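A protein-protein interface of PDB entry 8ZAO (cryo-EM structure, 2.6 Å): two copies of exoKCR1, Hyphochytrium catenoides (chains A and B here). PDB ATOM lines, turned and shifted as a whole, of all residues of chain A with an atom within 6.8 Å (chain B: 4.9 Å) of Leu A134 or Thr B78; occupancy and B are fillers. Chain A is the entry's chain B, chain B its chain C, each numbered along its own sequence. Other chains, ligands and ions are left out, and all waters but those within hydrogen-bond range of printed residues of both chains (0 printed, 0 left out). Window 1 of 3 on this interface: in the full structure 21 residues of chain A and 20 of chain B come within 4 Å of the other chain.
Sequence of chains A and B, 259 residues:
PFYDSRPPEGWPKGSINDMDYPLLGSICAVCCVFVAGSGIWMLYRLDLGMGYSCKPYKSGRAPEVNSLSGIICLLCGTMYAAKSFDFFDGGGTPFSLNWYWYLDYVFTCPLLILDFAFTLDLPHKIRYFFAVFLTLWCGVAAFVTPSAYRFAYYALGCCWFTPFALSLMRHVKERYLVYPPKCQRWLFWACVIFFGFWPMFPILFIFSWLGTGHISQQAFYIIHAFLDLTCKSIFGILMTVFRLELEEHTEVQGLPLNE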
ATOM      1  N   PRO A 110      21.680  19.583 -15.545  1.00  0.00           N
ATOM      2  CA  PRO A 110      20.750  18.845 -14.675  1.00  0.00           C
ATOM      3  C   PRO A 110      20.460  17.451 -15.197  1.00  0.00           C
ATOM      4  O   PRO A 110      20.417  16.486 -14.422  1.00  0.00           O
ATOM      5  CB  PRO A 110      19.500  19.734 -14.672  1.00  0.00           C
ATOM      6  CG  PRO A 110      20.013  21.089 -14.940  1.00  0.00           C
ATOM      7  CD  PRO A 110      21.133  20.901 -15.913  1.00  0.00           C
ATOM      8  N   PHE A 129      19.505  17.057  -8.986  1.00  0.00           N
ATOM      9  CA  PHE A 129      18.974  17.717 -10.173  1.00  0.00           C
ATOM     10  C   PHE A 129      18.663  19.178  -9.886  1.00  0.00           C
ATOM     11  O   PHE A 129      19.083  20.075 -10.628  1.00  0.00           O
ATOM     12  CB  PHE A 129      17.723  16.974 -10.651  1.00  0.00           C
ATOM     13  CG  PHE A 129      17.078  17.572 -11.872  1.00  0.00           C
ATOM     14  CD1 PHE A 129      16.141  18.585 -11.755  1.00  0.00           C
ATOM     15  CD2 PHE A 129      17.395  17.104 -13.134  1.00  0.00           C
ATOM     16  CE1 PHE A 129      15.546  19.130 -12.874  1.00  0.00           C
ATOM     17  CE2 PHE A 129      16.799  17.643 -14.255  1.00  0.00           C
ATOM     18  CZ  PHE A 129      15.875  18.657 -14.125  1.00  0.00           C
ATOM     19  N   PHE A 130      17.945  19.440  -8.794  1.00  0.00           N
ATOM     20  CA  PHE A 130      17.556  20.810  -8.485  1.00  0.00           C
ATOM     21  C   PHE A 130      18.738  21.646  -8.016  1.00  0.00           C
ATOM     22  O   PHE A 130      18.774  22.854  -8.267  1.00  0.00           O
ATOM     23  CB  PHE A 130      16.436  20.812  -7.450  1.00  0.00           C
ATOM     24  CG  PHE A 130      15.067  20.696  -8.053  1.00  0.00           C
ATOM     25  CD1 PHE A 130      14.515  21.755  -8.753  1.00  0.00           C
ATOM     26  CD2 PHE A 130      14.345  19.521  -7.949  1.00  0.00           C
ATOM     27  CE1 PHE A 130      13.261  21.650  -9.319  1.00  0.00           C
ATOM     28  CE2 PHE A 130      13.090  19.412  -8.511  1.00  0.00           C
ATOM     29  CZ  PHE A 130      12.548  20.476  -9.198  1.00  0.00           C
ATOM     30  N   ALA A 131      19.721  21.028  -7.357  1.00  0.00           N
ATOM     31  CA  ALA A 131      20.927  21.757  -6.980  1.00  0.00           C
ATOM     32  C   ALA A 131      21.669  22.255  -8.212  1.00  0.00           C
ATOM     33  O   ALA A 131      22.068  23.425  -8.283  1.00  0.00           O
ATOM     34  CB  ALA A 131      21.830  20.868  -6.126  1.00  0.00           C
ATOM     35  N   VAL A 132      21.849  21.383  -9.206  1.00  0.00           N
ATOM     36  CA  VAL A 132      22.524  21.797 -10.434  1.00  0.00           C
ATOM     37  C   VAL A 132      21.686  22.826 -11.187  1.00  0.00           C
ATOM     38  O   VAL A 132      22.218  23.798 -11.739  1.00  0.00           O
ATOM     39  CB  VAL A 132      22.847  20.571 -11.305  1.00  0.00           C
ATOM     40  CG1 VAL A 132      23.539  20.996 -12.587  1.00  0.00           C
ATOM     41  CG2 VAL A 132      23.724  19.604 -10.532  1.00  0.00           C
ATOM     42  N   PHE A 133      20.366  22.628 -11.220  1.00  0.00           N
ATOM     43  CA  PHE A 133      19.463  23.583 -11.855  1.00  0.00           C
ATOM     44  C   PHE A 133      19.626  24.979 -11.263  1.00  0.00           C
ATOM     45  O   PHE A 133      19.785  25.969 -11.990  1.00  0.00           O
ATOM     46  CB  PHE A 133      18.024  23.084 -11.687  1.00  0.00           C
ATOM     47  CG  PHE A 133      17.026  23.762 -12.575  1.00  0.00           C
ATOM     48  CD1 PHE A 133      17.019  23.530 -13.938  1.00  0.00           C
ATOM     49  CD2 PHE A 133      16.072  24.610 -12.041  1.00  0.00           C
ATOM     50  CE1 PHE A 133      16.093  24.144 -14.753  1.00  0.00           C
ATOM     51  CE2 PHE A 133      15.143  25.228 -12.851  1.00  0.00           C
ATOM     52  CZ  PHE A 133      15.152  24.991 -14.207  1.00  0.00           C
ATOM     53  N   LEU A 134      19.606  25.071  -9.932  1.00  0.00           N
ATOM     54  CA  LEU A 134      19.704  26.367  -9.273  1.00  0.00           C
ATOM     55  C   LEU A 134      21.095  26.967  -9.425  1.00  0.00           C
ATOM     56  O   LEU A 134      21.233  28.186  -9.570  1.00  0.00           O
ATOM     57  CB  LEU A 134      19.326  26.232  -7.800  1.00  0.00           C
ATOM     58  CG  LEU A 134      17.821  26.087  -7.573  1.00  0.00           C
ATOM     59  CD1 LEU A 134      17.483  26.090  -6.096  1.00  0.00           C
ATOM     60  CD2 LEU A 134      17.086  27.202  -8.291  1.00  0.00           C
ATOM     61  N   THR A 135      22.138  26.132  -9.403  1.00  0.00           N
ATOM     62  CA  THR A 135      23.487  26.642  -9.632  1.00  0.00           C
ATOM     63  C   THR A 135      23.606  27.273 -11.012  1.00  0.00           C
ATOM     64  O   THR A 135      24.162  28.368 -11.165  1.00  0.00           O
ATOM     65  CB  THR A 135      24.505  25.514  -9.475  1.00  0.00           C
ATOM     66  OG1 THR A 135      24.263  24.816  -8.249  1.00  0.00           O
ATOM     67  CG2 THR A 135      25.914  26.071  -9.460  1.00  0.00           C
ATOM     68  N   LEU A 136      23.070  26.601 -12.031  1.00  0.00           N
ATOM     69  CA  LEU A 136      23.142  27.137 -13.384  1.00  0.00           C
ATOM     70  C   LEU A 136      22.292  28.386 -13.553  1.00  0.00           C
ATOM     71  O   LEU A 136      22.692  29.305 -14.276  1.00  0.00           O
ATOM     72  CB  LEU A 136      22.718  26.073 -14.388  1.00  0.00           C
ATOM     73  CG  LEU A 136      23.712  24.923 -14.482  1.00  0.00           C
ATOM     74  CD1 LEU A 136      23.068  23.779 -15.208  1.00  0.00           C
ATOM     75  CD2 LEU A 136      24.982  25.371 -15.183  1.00  0.00           C
ATOM     76  N   TRP A 137      21.125  28.447 -12.915  1.00  0.00           N
ATOM     77  CA  TRP A 137      20.342  29.673 -12.984  1.00  0.00           C
ATOM     78  C   TRP A 137      21.017  30.834 -12.267  1.00  0.00           C
ATOM     79  O   TRP A 137      20.936  31.971 -12.744  1.00  0.00           O
ATOM     80  CB  TRP A 137      18.939  29.441 -12.429  1.00  0.00           C
ATOM     81  CG  TRP A 137      18.002  28.967 -13.485  1.00  0.00           C
ATOM     82  CD1 TRP A 137      17.403  27.749 -13.559  1.00  0.00           C
ATOM     83  CD2 TRP A 137      17.579  29.696 -14.643  1.00  0.00           C
ATOM     84  NE1 TRP A 137      16.620  27.675 -14.685  1.00  0.00           N
ATOM     85  CE2 TRP A 137      16.711  28.859 -15.367  1.00  0.00           C
ATOM     86  CE3 TRP A 137      17.843  30.979 -15.131  1.00  0.00           C
ATOM     87  CZ2 TRP A 137      16.107  29.260 -16.554  1.00  0.00           C
ATOM     88  CZ3 TRP A 137      17.242  31.374 -16.309  1.00  0.00           C
ATOM     89  CH2 TRP A 137      16.384  30.519 -17.007  1.00  0.00           C
ATOM     90  N   CYS A 138      21.691  30.574 -11.144  1.00  0.00           N
ATOM     91  CA  CYS A 138      22.505  31.603 -10.512  1.00  0.00           C
ATOM     92  C   CYS A 138      23.623  32.075 -11.431  1.00  0.00           C
ATOM     93  O   CYS A 138      23.917  33.273 -11.479  1.00  0.00           O
ATOM     94  CB  CYS A 138      23.088  31.081  -9.199  1.00  0.00           C
ATOM     95  SG  CYS A 138      21.864  30.760  -7.916  1.00  0.00           S
ATOM     96  N   GLY A 139      24.254  31.153 -12.161  1.00  0.00           N
ATOM     97  CA  GLY A 139      25.242  31.552 -13.148  1.00  0.00           C
ATOM     98  C   GLY A 139      24.684  32.405 -14.268  1.00  0.00           C
ATOM     99  O   GLY A 139      25.314  33.388 -14.674  1.00  0.00           O
ATOM    100  N   TYR A 153      25.102  36.876  -7.171  1.00  0.00           N
ATOM    101  CA  TYR A 153      24.542  35.714  -7.850  1.00  0.00           C
ATOM    102  C   TYR A 153      25.569  34.604  -7.978  1.00  0.00           C
ATOM    103  O   TYR A 153      25.278  33.451  -7.638  1.00  0.00           O
ATOM    104  CB  TYR A 153      24.032  36.106  -9.235  1.00  0.00           C
ATOM    105  CG  TYR A 153      22.710  36.836  -9.238  1.00  0.00           C
ATOM    106  CD1 TYR A 153      21.555  36.225  -8.772  1.00  0.00           C
ATOM    107  CD2 TYR A 153      22.618  38.134  -9.717  1.00  0.00           C
ATOM    108  CE1 TYR A 153      20.346  36.891  -8.782  1.00  0.00           C
ATOM    109  CE2 TYR A 153      21.415  38.806  -9.728  1.00  0.00           C
ATOM    110  CZ  TYR A 153      20.283  38.181  -9.260  1.00  0.00           C
ATOM    111  OH  TYR A 153      19.083  38.852  -9.272  1.00  0.00           O
ATOM    112  N   LEU A 156      25.795  33.094  -4.749  1.00  0.00           N
ATOM    113  CA  LEU A 156      24.648  32.216  -4.556  1.00  0.00           C
ATOM    114  C   LEU A 156      24.878  30.880  -5.244  1.00  0.00           C
ATOM    115  O   LEU A 156      24.646  29.821  -4.650  1.00  0.00           O
ATOM    116  CB  LEU A 156      23.378  32.888  -5.074  1.00  0.00           C
ATOM    117  CG  LEU A 156      22.046  32.259  -4.665  1.00  0.00           C
ATOM    118  CD1 LEU A 156      22.004  32.011  -3.166  1.00  0.00           C
ATOM    119  CD2 LEU A 156      20.888  33.139  -5.100  1.00  0.00           C
ATOM    120  N   GLY A 157      25.381  30.909  -6.482  1.00  0.00           N
ATOM    121  CA  GLY A 157      25.772  29.674  -7.130  1.00  0.00           C
ATOM    122  C   GLY A 157      26.836  28.913  -6.381  1.00  0.00           C
ATOM    123  O   GLY A 157      26.740  27.688  -6.264  1.00  0.00           O
ATOM    124  N   TRP A 160      25.533  26.802  -3.749  1.00  0.00           N
ATOM    125  CA  TRP A 160      24.882  25.577  -4.188  1.00  0.00           C
ATOM    126  C   TRP A 160      25.850  24.534  -4.707  1.00  0.00           C
ATOM    127  O   TRP A 160      25.661  23.347  -4.439  1.00  0.00           O
ATOM    128  CB  TRP A 160      23.864  25.882  -5.290  1.00  0.00           C
ATOM    129  CG  TRP A 160      22.499  26.113  -4.773  1.00  0.00           C
ATOM    130  CD1 TRP A 160      21.848  27.301  -4.704  1.00  0.00           C
ATOM    131  CD2 TRP A 160      21.606  25.129  -4.243  1.00  0.00           C
ATOM    132  NE1 TRP A 160      20.603  27.123  -4.166  1.00  0.00           N
ATOM    133  CE2 TRP A 160      20.428  25.798  -3.873  1.00  0.00           C
ATOM    134  CE3 TRP A 160      21.689  23.748  -4.046  1.00  0.00           C
ATOM    135  CZ2 TRP A 160      19.338  25.136  -3.316  1.00  0.00           C
ATOM    136  CZ3 TRP A 160      20.608  23.093  -3.495  1.00  0.00           C
ATOM    137  CH2 TRP A 160      19.447  23.786  -3.137  1.00  0.00           C
ATOM    138  N   LEU B  74      13.749  25.348  -0.517  1.00  0.00           N
ATOM    139  CA  LEU B  74      15.063  25.858  -0.893  1.00  0.00           C
ATOM    140  C   LEU B  74      15.023  26.635  -2.202  1.00  0.00           C
ATOM    141  O   LEU B  74      15.698  27.663  -2.329  1.00  0.00           O
ATOM    142  CB  LEU B  74      16.064  24.707  -0.991  1.00  0.00           C
ATOM    143  CG  LEU B  74      16.697  24.292   0.336  1.00  0.00           C
ATOM    144  CD1 LEU B  74      17.081  22.827   0.302  1.00  0.00           C
ATOM    145  CD2 LEU B  74      17.903  25.158   0.650  1.00  0.00           C
ATOM    146  N   LEU B  75      14.245  26.165  -3.178  1.00  0.00           N
ATOM    147  CA  LEU B  75      14.085  26.895  -4.430  1.00  0.00           C
ATOM    148  C   LEU B  75      13.439  28.254  -4.197  1.00  0.00           C
ATOM    149  O   LEU B  75      13.872  29.259  -4.774  1.00  0.00           O
ATOM    150  CB  LEU B  75      13.264  26.055  -5.408  1.00  0.00           C
ATOM    151  CG  LEU B  75      12.634  26.704  -6.639  1.00  0.00           C
ATOM    152  CD1 LEU B  75      13.583  26.665  -7.815  1.00  0.00           C
ATOM    153  CD2 LEU B  75      11.348  25.982  -6.986  1.00  0.00           C
ATOM    154  N   CYS B  76      12.415  28.311  -3.344  1.00  0.00           N
ATOM    155  CA  CYS B  76      11.788  29.586  -3.014  1.00  0.00           C
ATOM    156  C   CYS B  76      12.750  30.498  -2.264  1.00  0.00           C
ATOM    157  O   CYS B  76      12.761  31.712  -2.486  1.00  0.00           O
ATOM    158  CB  CYS B  76      10.520  29.348  -2.197  1.00  0.00           C
ATOM    159  SG  CYS B  76       9.744  30.845  -1.556  1.00  0.00           S
ATOM    160  N   GLY B  77      13.563  29.934  -1.370  1.00  0.00           N
ATOM    161  CA  GLY B  77      14.538  30.743  -0.658  1.00  0.00           C
ATOM    162  C   GLY B  77      15.590  31.332  -1.577  1.00  0.00           C
ATOM    163  O   GLY B  77      15.991  32.486  -1.418  1.00  0.00           O
ATOM    164  N   THR B  78      16.048  30.554  -2.557  1.00  0.00           N
ATOM    165  CA  THR B  78      17.004  31.092  -3.520  1.00  0.00           C
ATOM    166  C   THR B  78      16.353  32.108  -4.448  1.00  0.00           C
ATOM    167  O   THR B  78      16.988  33.102  -4.825  1.00  0.00           O
ATOM    168  CB  THR B  78      17.631  29.960  -4.323  1.00  0.00           C
ATOM    169  OG1 THR B  78      16.603  29.223  -4.993  1.00  0.00           O
ATOM    170  CG2 THR B  78      18.358  29.039  -3.385  1.00  0.00           C
ATOM    171  N   MET B  79      15.091  31.884  -4.819  1.00  0.00           N
ATOM    172  CA  MET B  79      14.361  32.889  -5.577  1.00  0.00           C
ATOM    173  C   MET B  79      14.234  34.184  -4.790  1.00  0.00           C
ATOM    174  O   MET B  79      14.334  35.268  -5.367  1.00  0.00           O
ATOM    175  CB  MET B  79      12.980  32.359  -5.962  1.00  0.00           C
ATOM    176  CG  MET B  79      13.001  31.357  -7.100  1.00  0.00           C
ATOM    177  SD  MET B  79      11.377  30.670  -7.459  1.00  0.00           S
ATOM    178  CE  MET B  79      11.511  30.411  -9.225  1.00  0.00           C
ATOM    179  N   TYR B  80      14.037  34.095  -3.475  1.00  0.00           N
ATOM    180  CA  TYR B  80      13.965  35.296  -2.654  1.00  0.00           C
ATOM    181  C   TYR B  80      15.329  35.934  -2.438  1.00  0.00           C
ATOM    182  O   TYR B  80      15.405  37.153  -2.270  1.00  0.00           O
ATOM    183  CB  TYR B  80      13.304  34.978  -1.315  1.00  0.00           C
ATOM    184  CG  TYR B  80      11.817  35.220  -1.340  1.00  0.00           C
ATOM    185  CD1 TYR B  80      11.308  36.508  -1.403  1.00  0.00           C
ATOM    186  CD2 TYR B  80      10.923  34.162  -1.338  1.00  0.00           C
ATOM    187  CE1 TYR B  80       9.950  36.735  -1.442  1.00  0.00           C
ATOM    188  CE2 TYR B  80       9.564  34.380  -1.377  1.00  0.00           C
ATOM    189  CZ  TYR B  80       9.083  35.668  -1.429  1.00  0.00           C
ATOM    190  OH  TYR B  80       7.729  35.887  -1.469  1.00  0.00           O
ATOM    191  N   ALA B  81      16.405  35.149  -2.442  1.00  0.00           N
ATOM    192  CA  ALA B  81      17.740  35.741  -2.463  1.00  0.00           C
ATOM    193  C   ALA B  81      17.954  36.546  -3.737  1.00  0.00           C
ATOM    194  O   ALA B  81      18.468  37.672  -3.694  1.00  0.00           O
ATOM    195  CB  ALA B  81      18.803  34.652  -2.330  1.00  0.00           C
ATOM    196  N   ALA B  82      17.549  35.990  -4.880  1.00  0.00           N
ATOM    197  CA  ALA B  82      17.612  36.736  -6.133  1.00  0.00           C
ATOM    198  C   ALA B  82      16.715  37.969  -6.098  1.00  0.00           C
ATOM    199  O   ALA B  82      17.084  39.020  -6.632  1.00  0.00           O
ATOM    200  CB  ALA B  82      17.228  35.831  -7.302  1.00  0.00           C
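Pro A110 touches none of the printed residues of chain B. Leu A134 touches two residues of chain B. Leu A136 touches none of the printed residues of chain B. Printed residues of chain B within 4 Å of Leu A156: Thr B78 (3.9 Å) and Ala B81 (3.8 Å). Of the printed residues of chain B, Trp A160 touches Thr B78 (3.1 Å). Of the printed residues of chain A, Leu B75 touches Leu A134. Thr B78 touches just these residues of chain A: Leu A134, Leu A156 and Trp A160. Of the printed residues of chain A, Ala B81 touches Leu A156. Of the printed residues of chain A, Ala B82 touches Tyr A153. The nearest residue of chain B that does not touch Leu A134 is Leu B74 (4.5 Å).
Among the printed residues, pairs that only touch across the chains: Leu A134 with Leu B75 (3.6 Å), Leu A134 with Thr B78 (3.4 Å), Leu A156 with Thr B78 (3.9 Å), Leu A156 with Ala B81 (3.8 Å) and Trp A160 with Thr B78 (3.1 Å).
No position is printed for both chains.
Of the 9 printed residues of chain B, 4 touch a printed residue of chain A. Hydrophobic or aromatic side chains of chain B within 4 Å of the printed part of chain A: Leu B75, Ala B81 and Ala B82. Hydrophobic or aromatic side chains of chain A that line the printed part of chain B: Leu A134, Tyr A153, Leu A156 and Trp A160. Among the printed residues, no Asp or Glu carboxylate lies within 4 Å of a Lys or Arg side-chain nitrogen of the other chain.
The backbone carbonyl oxygen of Leu A134 lies within hydrogen-bond range of the side-chain sulfur of Cys A138. The backbone carbonyl oxygen (O) of Leu B74 lies close to the side-chain hydroxyl (OG1) of Thr B78, at 3.2 Å. The backbone carbonyl oxygen of Leu B75 lies within hydrogen-bond range of the side-chain hydroxyl of Thr B78 (2.7 Å).
The side-chain hydroxyl (OH) of Tyr A153 is in hydrogen-bond range of the backbone carbonyl oxygen (O) of Ala B82.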
